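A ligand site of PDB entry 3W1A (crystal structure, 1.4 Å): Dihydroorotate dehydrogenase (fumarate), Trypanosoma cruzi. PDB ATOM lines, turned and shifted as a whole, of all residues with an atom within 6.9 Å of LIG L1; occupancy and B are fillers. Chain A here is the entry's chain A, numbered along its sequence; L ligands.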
ATOM      1  N   ALA A  20      21.710 -17.945 -32.966  1.00  0.00           N
ATOM      2  CA  ALA A  20      22.875 -18.646 -32.436  1.00  0.00           C
ATOM      3  C   ALA A  20      22.514 -20.019 -31.935  1.00  0.00           C
ATOM      4  O   ALA A  20      21.409 -20.248 -31.315  1.00  0.00           O
ATOM      5  CB  ALA A  20      23.498 -17.835 -31.322  1.00  0.00           C
ATOM      6  N   GLY A  21      23.361 -21.009 -32.182  1.00  0.00           N
ATOM      7  CA  GLY A  21      23.081 -22.379 -31.782  1.00  0.00           C
ATOM      8  C   GLY A  21      22.517 -23.261 -32.866  1.00  0.00           C
ATOM      9  O   GLY A  21      22.637 -24.478 -32.760  1.00  0.00           O
ATOM     10  N   LYS A  44      27.825 -20.871 -33.100  1.00  0.00           N
ATOM     11  CA  LYS A  44      27.304 -21.455 -31.829  1.00  0.00           C
ATOM     12  C   LYS A  44      27.970 -20.748 -30.651  1.00  0.00           C
ATOM     13  O   LYS A  44      29.208 -20.559 -30.638  1.00  0.00           O
ATOM     14  CB  LYS A  44      27.721 -22.937 -31.807  1.00  0.00           C
ATOM     15  CG  LYS A  44      27.565 -23.660 -30.430  1.00  0.00           C
ATOM     16  CD  LYS A  44      26.062 -23.730 -30.071  1.00  0.00           C
ATOM     17  CE  LYS A  44      25.925 -24.116 -28.575  1.00  0.00           C
ATOM     18  NZ  LYS A  44      24.423 -24.194 -28.294  1.00  0.00           N
ATOM     19  N   SER A  45      27.203 -20.445 -29.588  1.00  0.00           N
ATOM     20  CA  SER A  45      27.813 -19.823 -28.400  1.00  0.00           C
ATOM     21  C   SER A  45      28.928 -20.715 -27.880  1.00  0.00           C
ATOM     22  O   SER A  45      28.714 -21.960 -27.715  1.00  0.00           O
ATOM     23  CB  SER A  45      26.822 -19.679 -27.257  1.00  0.00           C
ATOM     24  OG  SER A  45      25.915 -18.593 -27.606  1.00  0.00           O
ATOM     25  N   ASN A  54      25.003 -31.255 -22.504  1.00  0.00           N
ATOM     26  CA  ASN A  54      24.126 -32.027 -21.593  1.00  0.00           C
ATOM     27  C   ASN A  54      23.732 -33.378 -22.238  1.00  0.00           C
ATOM     28  O   ASN A  54      23.889 -33.647 -23.403  1.00  0.00           O
ATOM     29  CB  ASN A  54      22.832 -31.261 -21.288  1.00  0.00           C
ATOM     30  CG  ASN A  54      23.012 -30.023 -20.476  1.00  0.00           C
ATOM     31  OD1 ASN A  54      24.025 -29.858 -19.724  1.00  0.00           O
ATOM     32  ND2 ASN A  54      22.049 -29.186 -20.491  1.00  0.00           N
ATOM     33  N   ASN A  68      14.705 -27.226 -25.706  1.00  0.00           N
ATOM     34  CA  ASN A  68      16.084 -27.657 -25.745  1.00  0.00           C
ATOM     35  C   ASN A  68      16.759 -27.416 -24.459  1.00  0.00           C
ATOM     36  O   ASN A  68      16.578 -26.402 -23.760  1.00  0.00           O
ATOM     37  CB  ASN A  68      16.924 -26.988 -26.909  1.00  0.00           C
ATOM     38  CG  ASN A  68      17.507 -25.655 -26.523  1.00  0.00           C
ATOM     39  OD1 ASN A  68      18.619 -25.592 -25.941  1.00  0.00           O
ATOM     40  ND2 ASN A  68      16.781 -24.562 -26.824  1.00  0.00           N
ATOM     41  N   SER A  69      17.624 -28.389 -24.124  1.00  0.00           N
ATOM     42  CA  SER A  69      18.663 -28.165 -23.044  1.00  0.00           C
ATOM     43  C   SER A  69      19.975 -28.659 -23.531  1.00  0.00           C
ATOM     44  O   SER A  69      20.536 -29.635 -23.036  1.00  0.00           O
ATOM     45  CB  SER A  69      18.213 -28.881 -21.725  1.00  0.00           C
ATOM     46  OG  SER A  69      19.165 -28.558 -20.673  1.00  0.00           O
ATOM     47  N   MET A  70      20.483 -27.963 -24.562  1.00  0.00           N
ATOM     48  CA  MET A  70      21.731 -28.467 -25.205  1.00  0.00           C
ATOM     49  C   MET A  70      22.905 -28.455 -24.223  1.00  0.00           C
ATOM     50  O   MET A  70      23.684 -29.448 -24.200  1.00  0.00           O
ATOM     51  CB  MET A  70      22.123 -27.645 -26.453  1.00  0.00           C
ATOM     52  CG  MET A  70      21.003 -27.470 -27.495  1.00  0.00           C
ATOM     53  SD  MET A  70      20.288 -29.033 -28.098  1.00  0.00           S
ATOM     54  CE  MET A  70      21.606 -29.582 -29.106  1.00  0.00           C
ATOM     55  N   GLY A  71      22.989 -27.409 -23.442  1.00  0.00           N
ATOM     56  CA  GLY A  71      24.108 -27.239 -22.479  1.00  0.00           C
ATOM     57  C   GLY A  71      25.415 -26.784 -23.040  1.00  0.00           C
ATOM     58  O   GLY A  71      26.501 -27.163 -22.561  1.00  0.00           O
ATOM     59  N   LEU A  72      25.299 -25.894 -24.028  1.00  0.00           N
ATOM     60  CA  LEU A  72      26.474 -25.250 -24.724  1.00  0.00           C
ATOM     61  C   LEU A  72      27.481 -26.330 -25.234  1.00  0.00           C
ATOM     62  O   LEU A  72      28.693 -26.150 -25.072  1.00  0.00           O
ATOM     63  CB  LEU A  72      27.207 -24.301 -23.803  1.00  0.00           C
ATOM     64  CG  LEU A  72      26.431 -23.001 -23.539  1.00  0.00           C
ATOM     65  CD1 LEU A  72      27.118 -22.186 -22.391  1.00  0.00           C
ATOM     66  CD2 LEU A  72      26.386 -22.092 -24.782  1.00  0.00           C
ATOM     67  N   PRO A  73      27.010 -27.372 -25.924  1.00  0.00           N
ATOM     68  CA  PRO A  73      27.977 -28.223 -26.632  1.00  0.00           C
ATOM     69  C   PRO A  73      28.621 -27.360 -27.712  1.00  0.00           C
ATOM     70  O   PRO A  73      27.912 -26.696 -28.485  1.00  0.00           O
ATOM     71  CB  PRO A  73      27.133 -29.342 -27.314  1.00  0.00           C
ATOM     72  CG  PRO A  73      25.732 -28.754 -27.401  1.00  0.00           C
ATOM     73  CD  PRO A  73      25.598 -27.621 -26.342  1.00  0.00           C
ATOM     74  N   SER A 100      29.648 -17.418 -24.784  1.00  0.00           N
ATOM     75  CA  SER A 100      28.841 -17.660 -23.595  1.00  0.00           C
ATOM     76  C   SER A 100      29.695 -18.270 -22.545  1.00  0.00           C
ATOM     77  O   SER A 100      29.418 -19.414 -22.111  1.00  0.00           O
ATOM     78  CB  SER A 100      27.626 -18.516 -24.029  1.00  0.00           C
ATOM     79  OG  SER A 100      26.664 -18.477 -22.992  1.00  0.00           O
ATOM     80  N   ASN A 128      26.493 -13.623 -25.133  1.00  0.00           N
ATOM     81  CA  ASN A 128      25.257 -14.296 -24.679  1.00  0.00           C
ATOM     82  C   ASN A 128      25.056 -14.198 -23.154  1.00  0.00           C
ATOM     83  O   ASN A 128      25.855 -14.812 -22.408  1.00  0.00           O
ATOM     84  CB  ASN A 128      25.353 -15.767 -25.126  1.00  0.00           C
ATOM     85  CG  ASN A 128      24.119 -16.589 -24.757  1.00  0.00           C
ATOM     86  OD1 ASN A 128      23.156 -16.078 -24.168  1.00  0.00           O
ATOM     87  ND2 ASN A 128      24.135 -17.831 -25.169  1.00  0.00           N
ATOM     88  N   SER A 130      22.188 -15.021 -21.648  1.00  0.00           N
ATOM     89  CA  SER A 130      20.870 -15.600 -21.470  1.00  0.00           C
ATOM     90  C   SER A 130      20.748 -17.125 -21.648  1.00  0.00           C
ATOM     91  O   SER A 130      19.700 -17.609 -21.802  1.00  0.00           O
ATOM     92  CB  SER A 130      19.854 -14.853 -22.354  1.00  0.00           C
ATOM     93  OG  SER A 130      20.317 -14.592 -23.656  1.00  0.00           O
ATOM     94  N   CYS A 131      21.849 -17.841 -21.586  1.00  0.00           N
ATOM     95  CA  CYS A 131      21.704 -19.328 -21.633  1.00  0.00           C
ATOM     96  C   CYS A 131      20.894 -19.758 -20.420  1.00  0.00           C
ATOM     97  O   CYS A 131      21.310 -19.521 -19.322  1.00  0.00           O
ATOM     98  CB  CYS A 131      23.109 -19.877 -21.630  1.00  0.00           C
ATOM     99  SG  CYS A 131      23.080 -21.731 -21.651  1.00  0.00           S
ATOM    100  N   PRO A 132      19.827 -20.552 -20.655  1.00  0.00           N
ATOM    101  CA  PRO A 132      19.030 -21.062 -19.539  1.00  0.00           C
ATOM    102  C   PRO A 132      19.194 -22.532 -19.250  1.00  0.00           C
ATOM    103  O   PRO A 132      18.354 -23.112 -18.527  1.00  0.00           O
ATOM    104  CB  PRO A 132      17.623 -20.798 -20.104  1.00  0.00           C
ATOM    105  CG  PRO A 132      17.712 -21.265 -21.620  1.00  0.00           C
ATOM    106  CD  PRO A 132      19.150 -20.818 -22.006  1.00  0.00           C
ATOM    107  N   ASN A 133      20.261 -23.140 -19.783  1.00  0.00           N
ATOM    108  CA  ASN A 133      20.364 -24.638 -19.750  1.00  0.00           C
ATOM    109  C   ASN A 133      21.611 -25.234 -19.152  1.00  0.00           C
ATOM    110  O   ASN A 133      21.746 -26.472 -19.154  1.00  0.00           O
ATOM    111  CB  ASN A 133      20.277 -25.171 -21.211  1.00  0.00           C
ATOM    112  CG  ASN A 133      18.973 -24.825 -21.900  1.00  0.00           C
ATOM    113  OD1 ASN A 133      17.920 -24.847 -21.269  1.00  0.00           O
ATOM    114  ND2 ASN A 133      19.021 -24.568 -23.211  1.00  0.00           N
ATOM    115  N   VAL A 134      22.493 -24.440 -18.539  1.00  0.00           N
ATOM    116  CA  VAL A 134      23.694 -25.043 -17.877  1.00  0.00           C
ATOM    117  C   VAL A 134      23.268 -25.209 -16.385  1.00  0.00           C
ATOM    118  O   VAL A 134      22.920 -24.206 -15.699  1.00  0.00           O
ATOM    119  CB  VAL A 134      24.908 -24.200 -18.052  1.00  0.00           C
ATOM    120  CG1 VAL A 134      26.070 -24.840 -17.229  1.00  0.00           C
ATOM    121  CG2 VAL A 134      25.303 -24.124 -19.506  1.00  0.00           C
ATOM    122  N   LYS A 165      22.949 -10.843 -26.414  1.00  0.00           N
ATOM    123  CA  LYS A 165      21.745 -11.723 -26.567  1.00  0.00           C
ATOM    124  C   LYS A 165      20.998 -11.762 -25.204  1.00  0.00           C
ATOM    125  O   LYS A 165      21.583 -12.243 -24.171  1.00  0.00           O
ATOM    126  CB  LYS A 165      22.218 -13.137 -26.889  1.00  0.00           C
ATOM    127  CG  LYS A 165      21.087 -14.135 -27.155  1.00  0.00           C
ATOM    128  CD  LYS A 165      20.276 -13.819 -28.435  1.00  0.00           C
ATOM    129  CE  LYS A 165      19.307 -15.016 -28.787  1.00  0.00           C
ATOM    130  NZ  LYS A 165      20.051 -16.203 -29.291  1.00  0.00           N
ATOM    131  N   ASN A 195      16.539 -14.718 -26.531  1.00  0.00           N
ATOM    132  CA  ASN A 195      16.851 -16.163 -26.322  1.00  0.00           C
ATOM    133  C   ASN A 195      15.603 -16.939 -25.986  1.00  0.00           C
ATOM    134  O   ASN A 195      14.470 -16.406 -25.909  1.00  0.00           O
ATOM    135  CB  ASN A 195      17.896 -16.177 -25.205  1.00  0.00           C
ATOM    136  CG  ASN A 195      18.887 -17.389 -25.290  1.00  0.00           C
ATOM    137  OD1 ASN A 195      18.488 -18.527 -25.625  1.00  0.00           O
ATOM    138  ND2 ASN A 195      20.211 -17.078 -25.193  1.00  0.00           N
ATOM    139  N   SER A 196      15.814 -18.278 -25.882  1.00  0.00           N
ATOM    140  CA  SER A 196      14.635 -19.113 -25.543  1.00  0.00           C
ATOM    141  C   SER A 196      13.932 -18.763 -24.251  1.00  0.00           C
ATOM    142  O   SER A 196      14.547 -18.146 -23.312  1.00  0.00           O
ATOM    143  CB  SER A 196      15.053 -20.607 -25.529  1.00  0.00           C
ATOM    144  OG  SER A 196      16.063 -20.828 -24.573  1.00  0.00           O
ATOM    145  N   VAL A 197      12.663 -19.044 -24.199  1.00  0.00           N
ATOM    146  CA  VAL A 197      11.900 -18.790 -22.982  1.00  0.00           C
ATOM    147  C   VAL A 197      12.234 -19.891 -21.946  1.00  0.00           C
ATOM    148  O   VAL A 197      11.929 -21.029 -22.169  1.00  0.00           O
ATOM    149  CB  VAL A 197      10.407 -18.700 -23.337  1.00  0.00           C
ATOM    150  CG1 VAL A 197       9.581 -18.766 -22.081  1.00  0.00           C
ATOM    151  CG2 VAL A 197      10.120 -17.418 -24.080  1.00  0.00           C
ATOM    152  N   GLY A 219      13.626 -27.140 -20.117  1.00  0.00           N
ATOM    153  CA  GLY A 219      14.462 -26.582 -21.167  1.00  0.00           C
ATOM    154  C   GLY A 219      13.848 -25.371 -21.733  1.00  0.00           C
ATOM    155  O   GLY A 219      12.702 -25.031 -21.511  1.00  0.00           O
ATOM    156  N   GLY A 220      14.662 -24.708 -22.585  1.00  0.00           N
ATOM    157  CA  GLY A 220      14.189 -23.428 -23.142  1.00  0.00           C
ATOM    158  C   GLY A 220      13.245 -23.633 -24.329  1.00  0.00           C
ATOM    159  O   GLY A 220      13.516 -24.562 -25.159  1.00  0.00           O
ATOM    160  N   LEU A 221      12.225 -22.806 -24.408  1.00  0.00           N
ATOM    161  CA  LEU A 221      11.223 -22.905 -25.525  1.00  0.00           C
ATOM    162  C   LEU A 221      11.539 -21.943 -26.629  1.00  0.00           C
ATOM    163  O   LEU A 221      11.854 -20.796 -26.405  1.00  0.00           O
ATOM    164  CB  LEU A 221       9.816 -22.570 -24.938  1.00  0.00           C
ATOM    165  CG  LEU A 221       9.416 -23.414 -23.699  1.00  0.00           C
ATOM    166  CD1 LEU A 221       8.129 -22.858 -23.130  1.00  0.00           C
ATOM    167  CD2 LEU A 221       9.254 -24.880 -24.064  1.00  0.00           C
HETATM  168  C1  LIG L   1      19.417 -22.023 -25.713  1.00  0.00           C
HETATM  169  C2  LIG L   1      21.301 -20.654 -25.274  1.00  0.00           C
HETATM  170  C3  LIG L   1      22.064 -21.835 -25.219  1.00  0.00           C
HETATM  171  O1  LIG L   1      18.157 -22.062 -25.944  1.00  0.00           O
HETATM  172  N1  LIG L   1      20.163 -23.133 -25.703  1.00  0.00           N
HETATM  173  N2  LIG L   1      19.981 -20.785 -25.459  1.00  0.00           N
HETATM  174  O2  LIG L   1      21.780 -19.541 -25.047  1.00  0.00           O
HETATM  175  F1  LIG L   1      23.347 -21.726 -25.048  1.00  0.00           F
HETATM  176  C4  LIG L   1      21.474 -23.086 -25.458  1.00  0.00           C
HETATM  177  C5  LIG L   1      22.232 -24.329 -25.209  1.00  0.00           C
HETATM  178  O3  LIG L   1      21.612 -25.066 -24.363  1.00  0.00           O
HETATM  179  O4  LIG L   1      23.383 -24.565 -25.622  1.00  0.00           O
HETATM  180  N1  LG2 L   2      20.906 -19.052 -28.207  1.00  0.00           N
HETATM  181  C1  LG2 L   2      22.165 -18.598 -28.059  1.00  0.00           C
HETATM  182  O1  LG2 L   2      22.349 -17.338 -27.855  1.00  0.00           O
HETATM  183  N2  LG2 L   2      23.303 -19.368 -28.099  1.00  0.00           N
HETATM  184  C2  LG2 L   2      23.218 -20.696 -28.330  1.00  0.00           C
HETATM  185  O2  LG2 L   2      24.285 -21.400 -28.514  1.00  0.00           O
HETATM  186  C3  LG2 L   2      21.916 -21.245 -28.540  1.00  0.00           C
HETATM  187  N3  LG2 L   2      21.813 -22.572 -28.841  1.00  0.00           N
HETATM  188  C4  LG2 L   2      20.574 -23.016 -29.244  1.00  0.00           C
HETATM  189  C5  LG2 L   2      20.399 -24.337 -29.636  1.00  0.00           C
HETATM  190  C6  LG2 L   2      19.147 -24.838 -30.036  1.00  0.00           C
HETATM  191  C7  LG2 L   2      19.100 -26.263 -30.535  1.00  0.00           C
HETATM  192  C8  LG2 L   2      18.050 -23.968 -30.004  1.00  0.00           C
HETATM  193  C9  LG2 L   2      16.697 -24.466 -30.444  1.00  0.00           C
HETATM  194  C10 LG2 L   2      18.160 -22.643 -29.583  1.00  0.00           C
HETATM  195  C11 LG2 L   2      19.436 -22.145 -29.212  1.00  0.00           C
HETATM  196  N4  LG2 L   2      19.549 -20.865 -28.737  1.00  0.00           N
HETATM  197  C12 LG2 L   2      20.808 -20.346 -28.493  1.00  0.00           C
HETATM  198  C13 LG2 L   2      18.393 -19.926 -28.722  1.00  0.00           C
HETATM  199  C14 LG2 L   2      18.088 -19.421 -30.119  1.00  0.00           C
HETATM  200  O3  LG2 L   2      19.213 -18.616 -30.593  1.00  0.00           O
HETATM  201  C15 LG2 L   2      16.856 -18.513 -30.140  1.00  0.00           C
HETATM  202  O4  LG2 L   2      17.145 -17.397 -29.259  1.00  0.00           O
HETATM  203  C16 LG2 L   2      15.595 -19.275 -29.598  1.00  0.00           C
HETATM  204  O5  LG2 L   2      15.605 -20.587 -30.098  1.00  0.00           O
HETATM  205  C17 LG2 L   2      14.350 -18.518 -30.038  1.00  0.00           C
HETATM  206  O6  LG2 L   2      14.175 -18.393 -31.438  1.00  0.00           O
HETATM  207  P1  LG2 L   2      13.189 -19.404 -32.253  1.00  0.00           P
HETATM  208  O7  LG2 L   2      11.805 -19.170 -31.715  1.00  0.00           O
HETATM  209  O8  LG2 L   2      13.660 -20.821 -31.980  1.00  0.00           O
HETATM  210  O9  LG2 L   2      13.423 -18.966 -33.698  1.00  0.00           O
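The backbone NH (N) of Met 70 sits at hydrogen-bond distance from an oxygen (O3) of LIG L1 (3.1 Å). O4 of LIG L1 lies within salt-bridge range of NZ of Lys 44. The side-chain amide nitrogen (ND2) of Asn 128 is in hydrogen-bond range of an oxygen (O1) of LG2 L2, 3.3 Å away. An oxygen (O3) of LIG L1 sits at hydrogen-bond distance from the side-chain amide nitrogen of Asn 133 (2.9 Å). The side-chain amino group (NZ) of Lys 44 is in hydrogen-bond range of an oxygen (O2) of LG2 L2. O2 of LG2 L2 is in hydrogen-bond range of N of Ser 45 (3.3 Å). O4 of LIG L1 lies within hydrogen-bond range of N of Leu 72, at 2.8 Å. O3 of LIG L1 sits at hydrogen-bond distance from N of Gly 71 (2.9 Å). The side-chain amide nitrogen (ND2) of Asn 128 lies within hydrogen-bond range of an oxygen (O2) of LIG L1, at 2.9 Å. The side-chain hydroxyl (OG) of Ser 196 sits at hydrogen-bond distance from an oxygen (O1) of LIG L1 (2.8 Å). OG of Ser 45 is in hydrogen-bond range of N2 of LG2 L2, 2.8 Å away. O3 of LG2 L2 sits at hydrogen-bond distance from NZ of Lys 165, 2.9 Å away. N2 of LIG L1 sits at hydrogen-bond distance from OD1 of Asn 195, 2.7 Å away. An oxygen (O1) of LG2 L2 is in hydrogen-bond range of the side-chain amide nitrogen (ND2) of Asn 195 (3.4 Å). An oxygen (O3) of LG2 L2 is in hydrogen-bond range of the backbone carbonyl oxygen (O) of Ala 20, at 2.8 Å. N1 of LIG L1 is in hydrogen-bond range of OD1 of Asn 68.
N1 of LG2 L2 lies close to N2 of LIG L1.
N of Asn 133 sits close to SG of Cys 131, 3.7 Å away. The backbone carbonyl oxygen of Met 70 sits at hydrogen-bond distance from the backbone NH of Asn 54. The side-chain amide nitrogen of Asn 195 is in hydrogen-bond range of the side-chain hydroxyl of Ser 130, 2.9 Å away. OD1 of Asn 68 is in hydrogen-bond range of ND2 of Asn 133 (2.9 Å). The side-chain amide nitrogen of Asn 128 is in hydrogen-bond range of the side-chain hydroxyl of Ser 100. O of Asn 68 sits at hydrogen-bond distance from N of Gly 220 (2.8 Å). N of Met 70 is in hydrogen-bond range of OD1 of Asn 68 (3.3 Å). N of Ser 130 is in hydrogen-bond range of OD1 of Asn 128 (2.9 Å).
The side-chain sulfur of Cys 131 sits close to a fluorine (F1) of LIG L1 (3.4 Å). Merely in contact with LIG L1: Pro 132 (3.6 Å) and Pro 73 (3.8 Å). Hydrophobic or aromatic side chains within 4 Å of LIG L1: Met 70, Leu 72, Pro 73 and Pro 132. Within 4 Å of LIG L1: Lys 44, Asn 68, Met 70, Gly 71, Leu 72, Pro 73, Asn 128, Cys 131, Pro 132, Asn 133, Asn 195 and Ser 196. The nearest printed residue that does not touch LIG L1 is Ser 69 (4.04 Å).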
